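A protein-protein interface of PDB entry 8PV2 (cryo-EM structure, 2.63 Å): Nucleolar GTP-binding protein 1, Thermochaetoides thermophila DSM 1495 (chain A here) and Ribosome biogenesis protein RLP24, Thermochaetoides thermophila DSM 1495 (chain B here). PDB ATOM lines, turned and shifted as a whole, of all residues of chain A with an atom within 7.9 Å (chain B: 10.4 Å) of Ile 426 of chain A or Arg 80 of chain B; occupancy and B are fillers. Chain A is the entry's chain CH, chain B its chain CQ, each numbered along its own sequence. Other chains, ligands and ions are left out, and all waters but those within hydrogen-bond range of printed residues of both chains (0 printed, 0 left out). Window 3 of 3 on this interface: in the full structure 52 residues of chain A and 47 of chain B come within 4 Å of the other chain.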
ATOM      1  N   ARG A 422      23.672  22.291   2.266  1.00  0.00           N
ATOM      2  CA  ARG A 422      23.345  21.413   3.376  1.00  0.00           C
ATOM      3  C   ARG A 422      23.009  19.998   2.937  1.00  0.00           C
ATOM      4  O   ARG A 422      22.654  19.172   3.780  1.00  0.00           O
ATOM      5  CB  ARG A 422      22.180  21.996   4.172  1.00  0.00           C
ATOM      6  CG  ARG A 422      22.582  23.124   5.092  1.00  0.00           C
ATOM      7  CD  ARG A 422      21.397  23.995   5.410  1.00  0.00           C
ATOM      8  NE  ARG A 422      21.697  24.988   6.432  1.00  0.00           N
ATOM      9  CZ  ARG A 422      21.317  24.891   7.695  1.00  0.00           C
ATOM     10  NH1 ARG A 422      20.653  23.836   8.136  1.00  0.00           N
ATOM     11  NH2 ARG A 422      21.602  25.878   8.536  1.00  0.00           N
ATOM     12  N   LYS A 423      23.115  19.703   1.641  1.00  0.00           N
ATOM     13  CA  LYS A 423      22.749  18.385   1.138  1.00  0.00           C
ATOM     14  C   LYS A 423      23.723  17.314   1.614  1.00  0.00           C
ATOM     15  O   LYS A 423      23.318  16.187   1.917  1.00  0.00           O
ATOM     16  CB  LYS A 423      22.688  18.419  -0.387  1.00  0.00           C
ATOM     17  CG  LYS A 423      22.246  17.125  -1.034  1.00  0.00           C
ATOM     18  CD  LYS A 423      22.092  17.298  -2.531  1.00  0.00           C
ATOM     19  CE  LYS A 423      23.442  17.459  -3.203  1.00  0.00           C
ATOM     20  NZ  LYS A 423      24.236  16.202  -3.155  1.00  0.00           N
ATOM     21  N   ASP A 424      25.009  17.650   1.694  1.00  0.00           N
ATOM     22  CA  ASP A 424      26.051  16.702   2.061  1.00  0.00           C
ATOM     23  C   ASP A 424      26.450  16.803   3.527  1.00  0.00           C
ATOM     24  O   ASP A 424      27.566  16.413   3.885  1.00  0.00           O
ATOM     25  CB  ASP A 424      27.275  16.899   1.170  1.00  0.00           C
ATOM     26  CG  ASP A 424      27.018  16.502  -0.265  1.00  0.00           C
ATOM     27  OD1 ASP A 424      25.939  15.940  -0.540  1.00  0.00           O
ATOM     28  OD2 ASP A 424      27.893  16.752  -1.119  1.00  0.00           O
ATOM     29  N   TRP A 425      25.573  17.325   4.377  1.00  0.00           N
ATOM     30  CA  TRP A 425      25.859  17.370   5.802  1.00  0.00           C
ATOM     31  C   TRP A 425      25.717  15.985   6.412  1.00  0.00           C
ATOM     32  O   TRP A 425      24.728  15.287   6.184  1.00  0.00           O
ATOM     33  CB  TRP A 425      24.926  18.352   6.503  1.00  0.00           C
ATOM     34  CG  TRP A 425      25.452  19.745   6.531  1.00  0.00           C
ATOM     35  CD1 TRP A 425      26.525  20.225   5.848  1.00  0.00           C
ATOM     36  CD2 TRP A 425      24.927  20.844   7.279  1.00  0.00           C
ATOM     37  NE1 TRP A 425      26.704  21.555   6.120  1.00  0.00           N
ATOM     38  CE2 TRP A 425      25.735  21.960   6.998  1.00  0.00           C
ATOM     39  CE3 TRP A 425      23.852  20.994   8.159  1.00  0.00           C
ATOM     40  CZ2 TRP A 425      25.505  23.208   7.567  1.00  0.00           C
ATOM     41  CZ3 TRP A 425      23.626  22.231   8.722  1.00  0.00           C
ATOM     42  CH2 TRP A 425      24.448  23.324   8.423  1.00  0.00           C
ATOM     43  N   ILE A 426      26.719  15.586   7.184  1.00  0.00           N
ATOM     44  CA  ILE A 426      26.729  14.309   7.883  1.00  0.00           C
ATOM     45  C   ILE A 426      26.292  14.588   9.312  1.00  0.00           C
ATOM     46  O   ILE A 426      27.088  15.066  10.127  1.00  0.00           O
ATOM     47  CB  ILE A 426      28.116  13.658   7.857  1.00  0.00           C
ATOM     48  CG1 ILE A 426      28.640  13.553   6.429  1.00  0.00           C
ATOM     49  CG2 ILE A 426      28.065  12.286   8.496  1.00  0.00           C
ATOM     50  CD1 ILE A 426      30.123  13.271   6.359  1.00  0.00           C
ATOM     51  N   LEU A 427      25.039  14.291   9.630  1.00  0.00           N
ATOM     52  CA  LEU A 427      24.512  14.573  10.954  1.00  0.00           C
ATOM     53  C   LEU A 427      23.996  13.302  11.609  1.00  0.00           C
ATOM     54  O   LEU A 427      23.828  12.266  10.963  1.00  0.00           O
ATOM     55  CB  LEU A 427      23.397  15.626  10.906  1.00  0.00           C
ATOM     56  CG  LEU A 427      23.790  17.001  10.368  1.00  0.00           C
ATOM     57  CD1 LEU A 427      22.638  17.963  10.514  1.00  0.00           C
ATOM     58  CD2 LEU A 427      25.013  17.535  11.075  1.00  0.00           C
ATOM     59  N   GLU A 428      23.766  13.401  12.919  1.00  0.00           N
ATOM     60  CA  GLU A 428      23.276  12.259  13.683  1.00  0.00           C
ATOM     61  C   GLU A 428      21.864  11.878  13.263  1.00  0.00           C
ATOM     62  O   GLU A 428      21.532  10.691  13.179  1.00  0.00           O
ATOM     63  CB  GLU A 428      23.323  12.570  15.179  1.00  0.00           C
ATOM     64  CG  GLU A 428      24.690  13.008  15.699  1.00  0.00           C
ATOM     65  CD  GLU A 428      24.853  14.522  15.760  1.00  0.00           C
ATOM     66  OE1 GLU A 428      24.304  15.224  14.885  1.00  0.00           O
ATOM     67  OE2 GLU A 428      25.535  15.011  16.687  1.00  0.00           O
ATOM     68  N   ASN A 429      21.016  12.869  13.005  1.00  0.00           N
ATOM     69  CA  ASN A 429      19.633  12.636  12.624  1.00  0.00           C
ATOM     70  C   ASN A 429      19.389  13.322  11.287  1.00  0.00           C
ATOM     71  O   ASN A 429      19.575  14.546  11.188  1.00  0.00           O
ATOM     72  CB  ASN A 429      18.696  13.177  13.701  1.00  0.00           C
ATOM     73  CG  ASN A 429      17.305  12.617  13.603  1.00  0.00           C
ATOM     74  OD1 ASN A 429      17.056  11.676  12.861  1.00  0.00           O
ATOM     75  ND2 ASN A 429      16.387  13.184  14.371  1.00  0.00           N
ATOM     76  N   PRO A 430      19.002  12.592  10.235  1.00  0.00           N
ATOM     77  CA  PRO A 430      19.019  13.173   8.878  1.00  0.00           C
ATOM     78  C   PRO A 430      18.030  14.304   8.630  1.00  0.00           C
ATOM     79  O   PRO A 430      18.212  15.041   7.654  1.00  0.00           O
ATOM     80  CB  PRO A 430      18.711  11.966   7.984  1.00  0.00           C
ATOM     81  CG  PRO A 430      19.140  10.793   8.783  1.00  0.00           C
ATOM     82  CD  PRO A 430      18.806  11.134  10.197  1.00  0.00           C
ATOM     83  N   TRP A 432      17.637  16.910  10.514  1.00  0.00           N
ATOM     84  CA  TRP A 432      18.165  18.141  11.079  1.00  0.00           C
ATOM     85  C   TRP A 432      18.946  18.982  10.084  1.00  0.00           C
ATOM     86  O   TRP A 432      19.312  20.113  10.414  1.00  0.00           O
ATOM     87  CB  TRP A 432      19.071  17.844  12.274  1.00  0.00           C
ATOM     88  CG  TRP A 432      18.423  17.199  13.438  1.00  0.00           C
ATOM     89  CD1 TRP A 432      17.092  17.103  13.692  1.00  0.00           C
ATOM     90  CD2 TRP A 432      19.088  16.581  14.539  1.00  0.00           C
ATOM     91  NE1 TRP A 432      16.883  16.453  14.881  1.00  0.00           N
ATOM     92  CE2 TRP A 432      18.096  16.124  15.422  1.00  0.00           C
ATOM     93  CE3 TRP A 432      20.430  16.367  14.863  1.00  0.00           C
ATOM     94  CZ2 TRP A 432      18.400  15.461  16.603  1.00  0.00           C
ATOM     95  CZ3 TRP A 432      20.729  15.709  16.033  1.00  0.00           C
ATOM     96  CH2 TRP A 432      19.720  15.264  16.891  1.00  0.00           C
ATOM     97  N   LYS A 433      19.220  18.473   8.881  1.00  0.00           N
ATOM     98  CA  LYS A 433      20.182  19.152   8.021  1.00  0.00           C
ATOM     99  C   LYS A 433      19.615  20.404   7.369  1.00  0.00           C
ATOM    100  O   LYS A 433      20.384  21.194   6.816  1.00  0.00           O
ATOM    101  CB  LYS A 433      20.724  18.204   6.952  1.00  0.00           C
ATOM    102  CG  LYS A 433      19.711  17.694   5.961  1.00  0.00           C
ATOM    103  CD  LYS A 433      20.410  16.986   4.812  1.00  0.00           C
ATOM    104  CE  LYS A 433      21.026  15.675   5.248  1.00  0.00           C
ATOM    105  NZ  LYS A 433      21.626  14.946   4.100  1.00  0.00           N
ATOM    106  N   ILE A 437      19.793  27.190  12.231  1.00  0.00           N
ATOM    107  CA  ILE A 437      20.627  27.080  13.423  1.00  0.00           C
ATOM    108  C   ILE A 437      20.647  28.423  14.145  1.00  0.00           C
ATOM    109  O   ILE A 437      21.007  29.440  13.536  1.00  0.00           O
ATOM    110  CB  ILE A 437      22.040  26.611  13.048  1.00  0.00           C
ATOM    111  CG1 ILE A 437      21.957  25.313  12.242  1.00  0.00           C
ATOM    112  CG2 ILE A 437      22.878  26.398  14.285  1.00  0.00           C
ATOM    113  CD1 ILE A 437      23.257  24.899  11.618  1.00  0.00           C
ATOM    114  N   ILE A 450      27.757  27.117  23.076  1.00  0.00           N
ATOM    115  CA  ILE A 450      27.703  25.719  22.658  1.00  0.00           C
ATOM    116  C   ILE A 450      28.875  24.966  23.268  1.00  0.00           C
ATOM    117  O   ILE A 450      30.041  25.288  23.018  1.00  0.00           O
ATOM    118  CB  ILE A 450      27.698  25.601  21.133  1.00  0.00           C
ATOM    119  CG1 ILE A 450      26.383  26.122  20.571  1.00  0.00           C
ATOM    120  CG2 ILE A 450      27.900  24.157  20.714  1.00  0.00           C
ATOM    121  CD1 ILE A 450      25.195  25.304  20.980  1.00  0.00           C
ATOM    122  N   ARG B  75      34.951  29.456  20.898  1.00  0.00           N
ATOM    123  CA  ARG B  75      35.083  28.024  20.656  1.00  0.00           C
ATOM    124  C   ARG B  75      35.827  27.810  19.346  1.00  0.00           C
ATOM    125  O   ARG B  75      35.264  27.998  18.263  1.00  0.00           O
ATOM    126  CB  ARG B  75      33.715  27.352  20.622  1.00  0.00           C
ATOM    127  CG  ARG B  75      32.788  27.800  21.722  1.00  0.00           C
ATOM    128  CD  ARG B  75      33.205  27.247  23.064  1.00  0.00           C
ATOM    129  NE  ARG B  75      32.290  27.673  24.114  1.00  0.00           N
ATOM    130  CZ  ARG B  75      32.337  27.247  25.366  1.00  0.00           C
ATOM    131  NH1 ARG B  75      33.254  26.384  25.767  1.00  0.00           N
ATOM    132  NH2 ARG B  75      31.444  27.701  26.239  1.00  0.00           N
ATOM    133  N   VAL B  77      37.166  24.854  18.476  1.00  0.00           N
ATOM    134  CA  VAL B  77      36.922  23.494  18.005  1.00  0.00           C
ATOM    135  C   VAL B  77      35.428  23.354  17.745  1.00  0.00           C
ATOM    136  O   VAL B  77      34.642  23.324  18.700  1.00  0.00           O
ATOM    137  CB  VAL B  77      37.417  22.449  19.012  1.00  0.00           C
ATOM    138  CG1 VAL B  77      37.120  21.059  18.506  1.00  0.00           C
ATOM    139  CG2 VAL B  77      38.900  22.616  19.248  1.00  0.00           C
ATOM    140  N   PRO B  78      34.996  23.290  16.488  1.00  0.00           N
ATOM    141  CA  PRO B  78      33.560  23.227  16.201  1.00  0.00           C
ATOM    142  C   PRO B  78      32.932  21.918  16.650  1.00  0.00           C
ATOM    143  O   PRO B  78      33.588  20.878  16.737  1.00  0.00           O
ATOM    144  CB  PRO B  78      33.498  23.374  14.677  1.00  0.00           C
ATOM    145  CG  PRO B  78      34.838  22.953  14.205  1.00  0.00           C
ATOM    146  CD  PRO B  78      35.793  23.404  15.257  1.00  0.00           C
ATOM    147  N   VAL B  79      31.638  21.989  16.941  1.00  0.00           N
ATOM    148  CA  VAL B  79      30.826  20.839  17.308  1.00  0.00           C
ATOM    149  C   VAL B  79      29.834  20.585  16.183  1.00  0.00           C
ATOM    150  O   VAL B  79      29.238  21.527  15.649  1.00  0.00           O
ATOM    151  CB  VAL B  79      30.105  21.080  18.649  1.00  0.00           C
ATOM    152  CG1 VAL B  79      29.220  19.904  19.020  1.00  0.00           C
ATOM    153  CG2 VAL B  79      31.113  21.344  19.747  1.00  0.00           C
ATOM    154  N   ARG B  80      29.692  19.318  15.799  1.00  0.00           N
ATOM    155  CA  ARG B  80      28.684  18.919  14.825  1.00  0.00           C
ATOM    156  C   ARG B  80      27.294  19.305  15.314  1.00  0.00           C
ATOM    157  O   ARG B  80      26.979  19.163  16.498  1.00  0.00           O
ATOM    158  CB  ARG B  80      28.767  17.413  14.587  1.00  0.00           C
ATOM    159  CG  ARG B  80      27.926  16.895  13.452  1.00  0.00           C
ATOM    160  CD  ARG B  80      28.279  15.457  13.157  1.00  0.00           C
ATOM    161  NE  ARG B  80      29.711  15.290  12.957  1.00  0.00           N
ATOM    162  CZ  ARG B  80      30.322  15.432  11.790  1.00  0.00           C
ATOM    163  NH1 ARG B  80      29.650  15.729  10.691  1.00  0.00           N
ATOM    164  NH2 ARG B  80      31.639  15.270  11.723  1.00  0.00           N
ATOM    165  N   TYR B  81      26.469  19.816  14.399  1.00  0.00           N
ATOM    166  CA  TYR B  81      25.199  20.418  14.782  1.00  0.00           C
ATOM    167  C   TYR B  81      24.239  19.372  15.331  1.00  0.00           C
ATOM    168  O   TYR B  81      24.116  18.273  14.784  1.00  0.00           O
ATOM    169  CB  TYR B  81      24.564  21.141  13.595  1.00  0.00           C
ATOM    170  CG  TYR B  81      23.114  21.510  13.827  1.00  0.00           C
ATOM    171  CD1 TYR B  81      22.772  22.537  14.693  1.00  0.00           C
ATOM    172  CD2 TYR B  81      22.090  20.829  13.185  1.00  0.00           C
ATOM    173  CE1 TYR B  81      21.460  22.874  14.913  1.00  0.00           C
ATOM    174  CE2 TYR B  81      20.776  21.156  13.404  1.00  0.00           C
ATOM    175  CZ  TYR B  81      20.465  22.179  14.269  1.00  0.00           C
ATOM    176  OH  TYR B  81      19.152  22.514  14.483  1.00  0.00           O
ATOM    177  N   ASN B  82      23.559  19.726  16.416  1.00  0.00           N
ATOM    178  CA  ASN B  82      22.639  18.831  17.102  1.00  0.00           C
ATOM    179  C   ASN B  82      21.496  19.677  17.639  1.00  0.00           C
ATOM    180  O   ASN B  82      21.721  20.563  18.470  1.00  0.00           O
ATOM    181  CB  ASN B  82      23.359  18.081  18.229  1.00  0.00           C
ATOM    182  CG  ASN B  82      22.555  16.922  18.782  1.00  0.00           C
ATOM    183  OD1 ASN B  82      21.362  17.037  19.053  1.00  0.00           O
ATOM    184  ND2 ASN B  82      23.216  15.789  18.958  1.00  0.00           N
ATOM    185  N   ARG B  83      20.277  19.391  17.171  1.00  0.00           N
ATOM    186  CA  ARG B  83      19.123  20.210  17.531  1.00  0.00           C
ATOM    187  C   ARG B  83      18.874  20.196  19.035  1.00  0.00           C
ATOM    188  O   ARG B  83      18.638  21.249  19.639  1.00  0.00           O
ATOM    189  CB  ARG B  83      17.882  19.725  16.783  1.00  0.00           C
ATOM    190  CG  ARG B  83      16.648  20.567  17.052  1.00  0.00           C
ATOM    191  CD  ARG B  83      15.397  19.963  16.452  1.00  0.00           C
ATOM    192  NE  ARG B  83      15.470  19.840  15.004  1.00  0.00           N
ATOM    193  CZ  ARG B  83      14.548  19.248  14.259  1.00  0.00           C
ATOM    194  NH1 ARG B  83      13.464  18.716  14.795  1.00  0.00           N
ATOM    195  NH2 ARG B  83      14.720  19.185  12.943  1.00  0.00           N
ATOM    196  N   GLU B  84      18.968  19.017  19.655  1.00  0.00           N
ATOM    197  CA  GLU B  84      18.757  18.899  21.095  1.00  0.00           C
ATOM    198  C   GLU B  84      19.800  19.687  21.877  1.00  0.00           C
ATOM    199  O   GLU B  84      19.479  20.337  22.883  1.00  0.00           O
ATOM    200  CB  GLU B  84      18.793  17.427  21.493  1.00  0.00           C
ATOM    201  CG  GLU B  84      17.647  16.614  20.929  1.00  0.00           C
ATOM    202  CD  GLU B  84      17.728  15.154  21.313  1.00  0.00           C
ATOM    203  OE1 GLU B  84      18.745  14.751  21.914  1.00  0.00           O
ATOM    204  OE2 GLU B  84      16.776  14.406  21.011  1.00  0.00           O
ATOM    205  N   LEU B  85      21.053  19.645  21.415  1.00  0.00           N
ATOM    206  CA  LEU B  85      22.119  20.392  22.069  1.00  0.00           C
ATOM    207  C   LEU B  85      21.874  21.892  21.978  1.00  0.00           C
ATOM    208  O   LEU B  85      22.076  22.617  22.957  1.00  0.00           O
ATOM    209  CB  LEU B  85      23.465  20.022  21.451  1.00  0.00           C
ATOM    210  CG  LEU B  85      24.678  20.832  21.906  1.00  0.00           C
ATOM    211  CD1 LEU B  85      24.926  20.614  23.384  1.00  0.00           C
ATOM    212  CD2 LEU B  85      25.903  20.464  21.097  1.00  0.00           C
ATOM    213  N   TRP B  86      21.419  22.372  20.819  1.00  0.00           N
ATOM    214  CA  TRP B  86      21.125  23.799  20.679  1.00  0.00           C
ATOM    215  C   TRP B  86      19.952  24.249  21.555  1.00  0.00           C
ATOM    216  O   TRP B  86      20.014  25.331  22.155  1.00  0.00           O
ATOM    217  CB  TRP B  86      20.910  24.144  19.205  1.00  0.00           C
ATOM    218  CG  TRP B  86      22.145  24.721  18.524  1.00  0.00           C
ATOM    219  CD1 TRP B  86      22.331  26.024  18.170  1.00  0.00           C
ATOM    220  CD2 TRP B  86      23.377  24.050  18.206  1.00  0.00           C
ATOM    221  NE1 TRP B  86      23.568  26.197  17.610  1.00  0.00           N
ATOM    222  CE2 TRP B  86      24.232  25.001  17.623  1.00  0.00           C
ATOM    223  CE3 TRP B  86      23.833  22.740  18.344  1.00  0.00           C
ATOM    224  CZ2 TRP B  86      25.509  24.683  17.180  1.00  0.00           C
ATOM    225  CZ3 TRP B  86      25.098  22.427  17.899  1.00  0.00           C
ATOM    226  CH2 TRP B  86      25.921  23.392  17.326  1.00  0.00           C
ATOM    227  N   LYS B  88      18.912  22.817  24.468  1.00  0.00           N
ATOM    228  CA  LYS B  88      19.348  22.837  25.861  1.00  0.00           C
ATOM    229  C   LYS B  88      20.369  23.943  26.108  1.00  0.00           C
ATOM    230  O   LYS B  88      20.424  24.491  27.215  1.00  0.00           O
ATOM    231  CB  LYS B  88      19.893  21.471  26.287  1.00  0.00           C
ATOM    232  CG  LYS B  88      21.228  21.069  25.701  1.00  0.00           C
ATOM    233  CD  LYS B  88      21.755  19.821  26.385  1.00  0.00           C
ATOM    234  CE  LYS B  88      20.974  18.578  25.992  1.00  0.00           C
ATOM    235  NZ  LYS B  88      21.223  18.168  24.587  1.00  0.00           N
ATOM    236  N   THR B  89      21.133  24.328  25.082  1.00  0.00           N
ATOM    237  CA  THR B  89      22.020  25.479  25.207  1.00  0.00           C
ATOM    238  C   THR B  89      21.235  26.770  25.393  1.00  0.00           C
ATOM    239  O   THR B  89      21.614  27.611  26.210  1.00  0.00           O
ATOM    240  CB  THR B  89      22.931  25.579  23.985  1.00  0.00           C
ATOM    241  OG1 THR B  89      23.651  24.352  23.826  1.00  0.00           O
ATOM    242  CG2 THR B  89      23.919  26.717  24.146  1.00  0.00           C
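Printed residues of chain B that touch a printed residue of chain A: Arg 75, Arg 80, Tyr 81, Asn 82, Arg 83, Trp 86 and Thr 89.
Of chain B, only Arg 80 comes within 4 Å of Ile 426 of chain A.
Of chain B, only Arg 80 and Tyr 81 come within 4 Å of Leu 427 of chain A.
Printed residues of chain B within 4 Å of Glu 428 of chain A: Tyr 81 (3.1 Å) and Asn 82 (3.3 Å).
Of the printed residues of chain B, Ile 450 of chain A touches Arg 75, Trp 86 and Thr 89.
Printed residues of chain A within 4 Å of Arg 75 of chain B: Ile 450.
Of chain A, only Ile 426 and Leu 427 come within 4 Å of Arg 80 of chain B.
The nearest residue of chain B that does not touch Ile 426 of chain A is Tyr 81 of chain B (6.4 Å).
The nearest residue of chain A that does not touch Arg 80 of chain B is Glu 428 of chain A (4.2 Å).
The nearest printed residue of chain A that does not touch Tyr 81 of chain B is Trp 425 of chain A (4.9 Å).
Leu 427 of chain A touches Arg 80 of chain B (CD2 to CG, 3.8 Å).
Leu 427 of chain A touches Tyr 81 of chain B.
Tyr 81 of chain B touches Trp 432 of chain A (CE2 to O, 3.5 Å).
Trp 432 of chain A touches Asn 82 of chain B (CH2 to OD1, 3.2 Å).
Arg 83 of chain B touches Trp 432 of chain A.
Tyr 81 of chain B touches Ile 437 of chain A (CE1 to CG1, 3.7 Å).
CG2 of Ile 437 of chain A touches NE1 of Trp 86 of chain B (3.4 Å).
CE2 of Trp 86 of chain B touches CD1 of Ile 450 of chain A (3.5 Å).
CD1 of Ile 450 of chain A touches OG1 of Thr 89 of chain B, 3.4 Å away.
The side-chain amide oxygen (OD1) of Asn 82 of chain B is in hydrogen-bond range of the backbone NH (N) of Glu 84 of chain B (3.2 Å).
OG1 of Thr 89 of chain B sits at hydrogen-bond distance from O of Leu 85 of chain B.
The indole nitrogen (NE1) of Trp 432 of chain A sits close to the side-chain amide nitrogen (ND2) of Asn 429 of chain A.
The guanidinium group (NE) of Arg 75 of chain B is in hydrogen-bond range of the backbone carbonyl oxygen (O) of Ile 450 of chain A.
O of Ile 426 of chain A is in hydrogen-bond range of NH1 of Arg 80 of chain B, at 2.7 Å.
ND2 of Asn 82 of chain B sits at hydrogen-bond distance from OE2 of Glu 428 of chain A (3.3 Å).
The side-chain carboxylate (OE1) of Glu 428 of chain A lies close to the backbone carbonyl oxygen (O) of Tyr 81 of chain B (3.1 Å).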
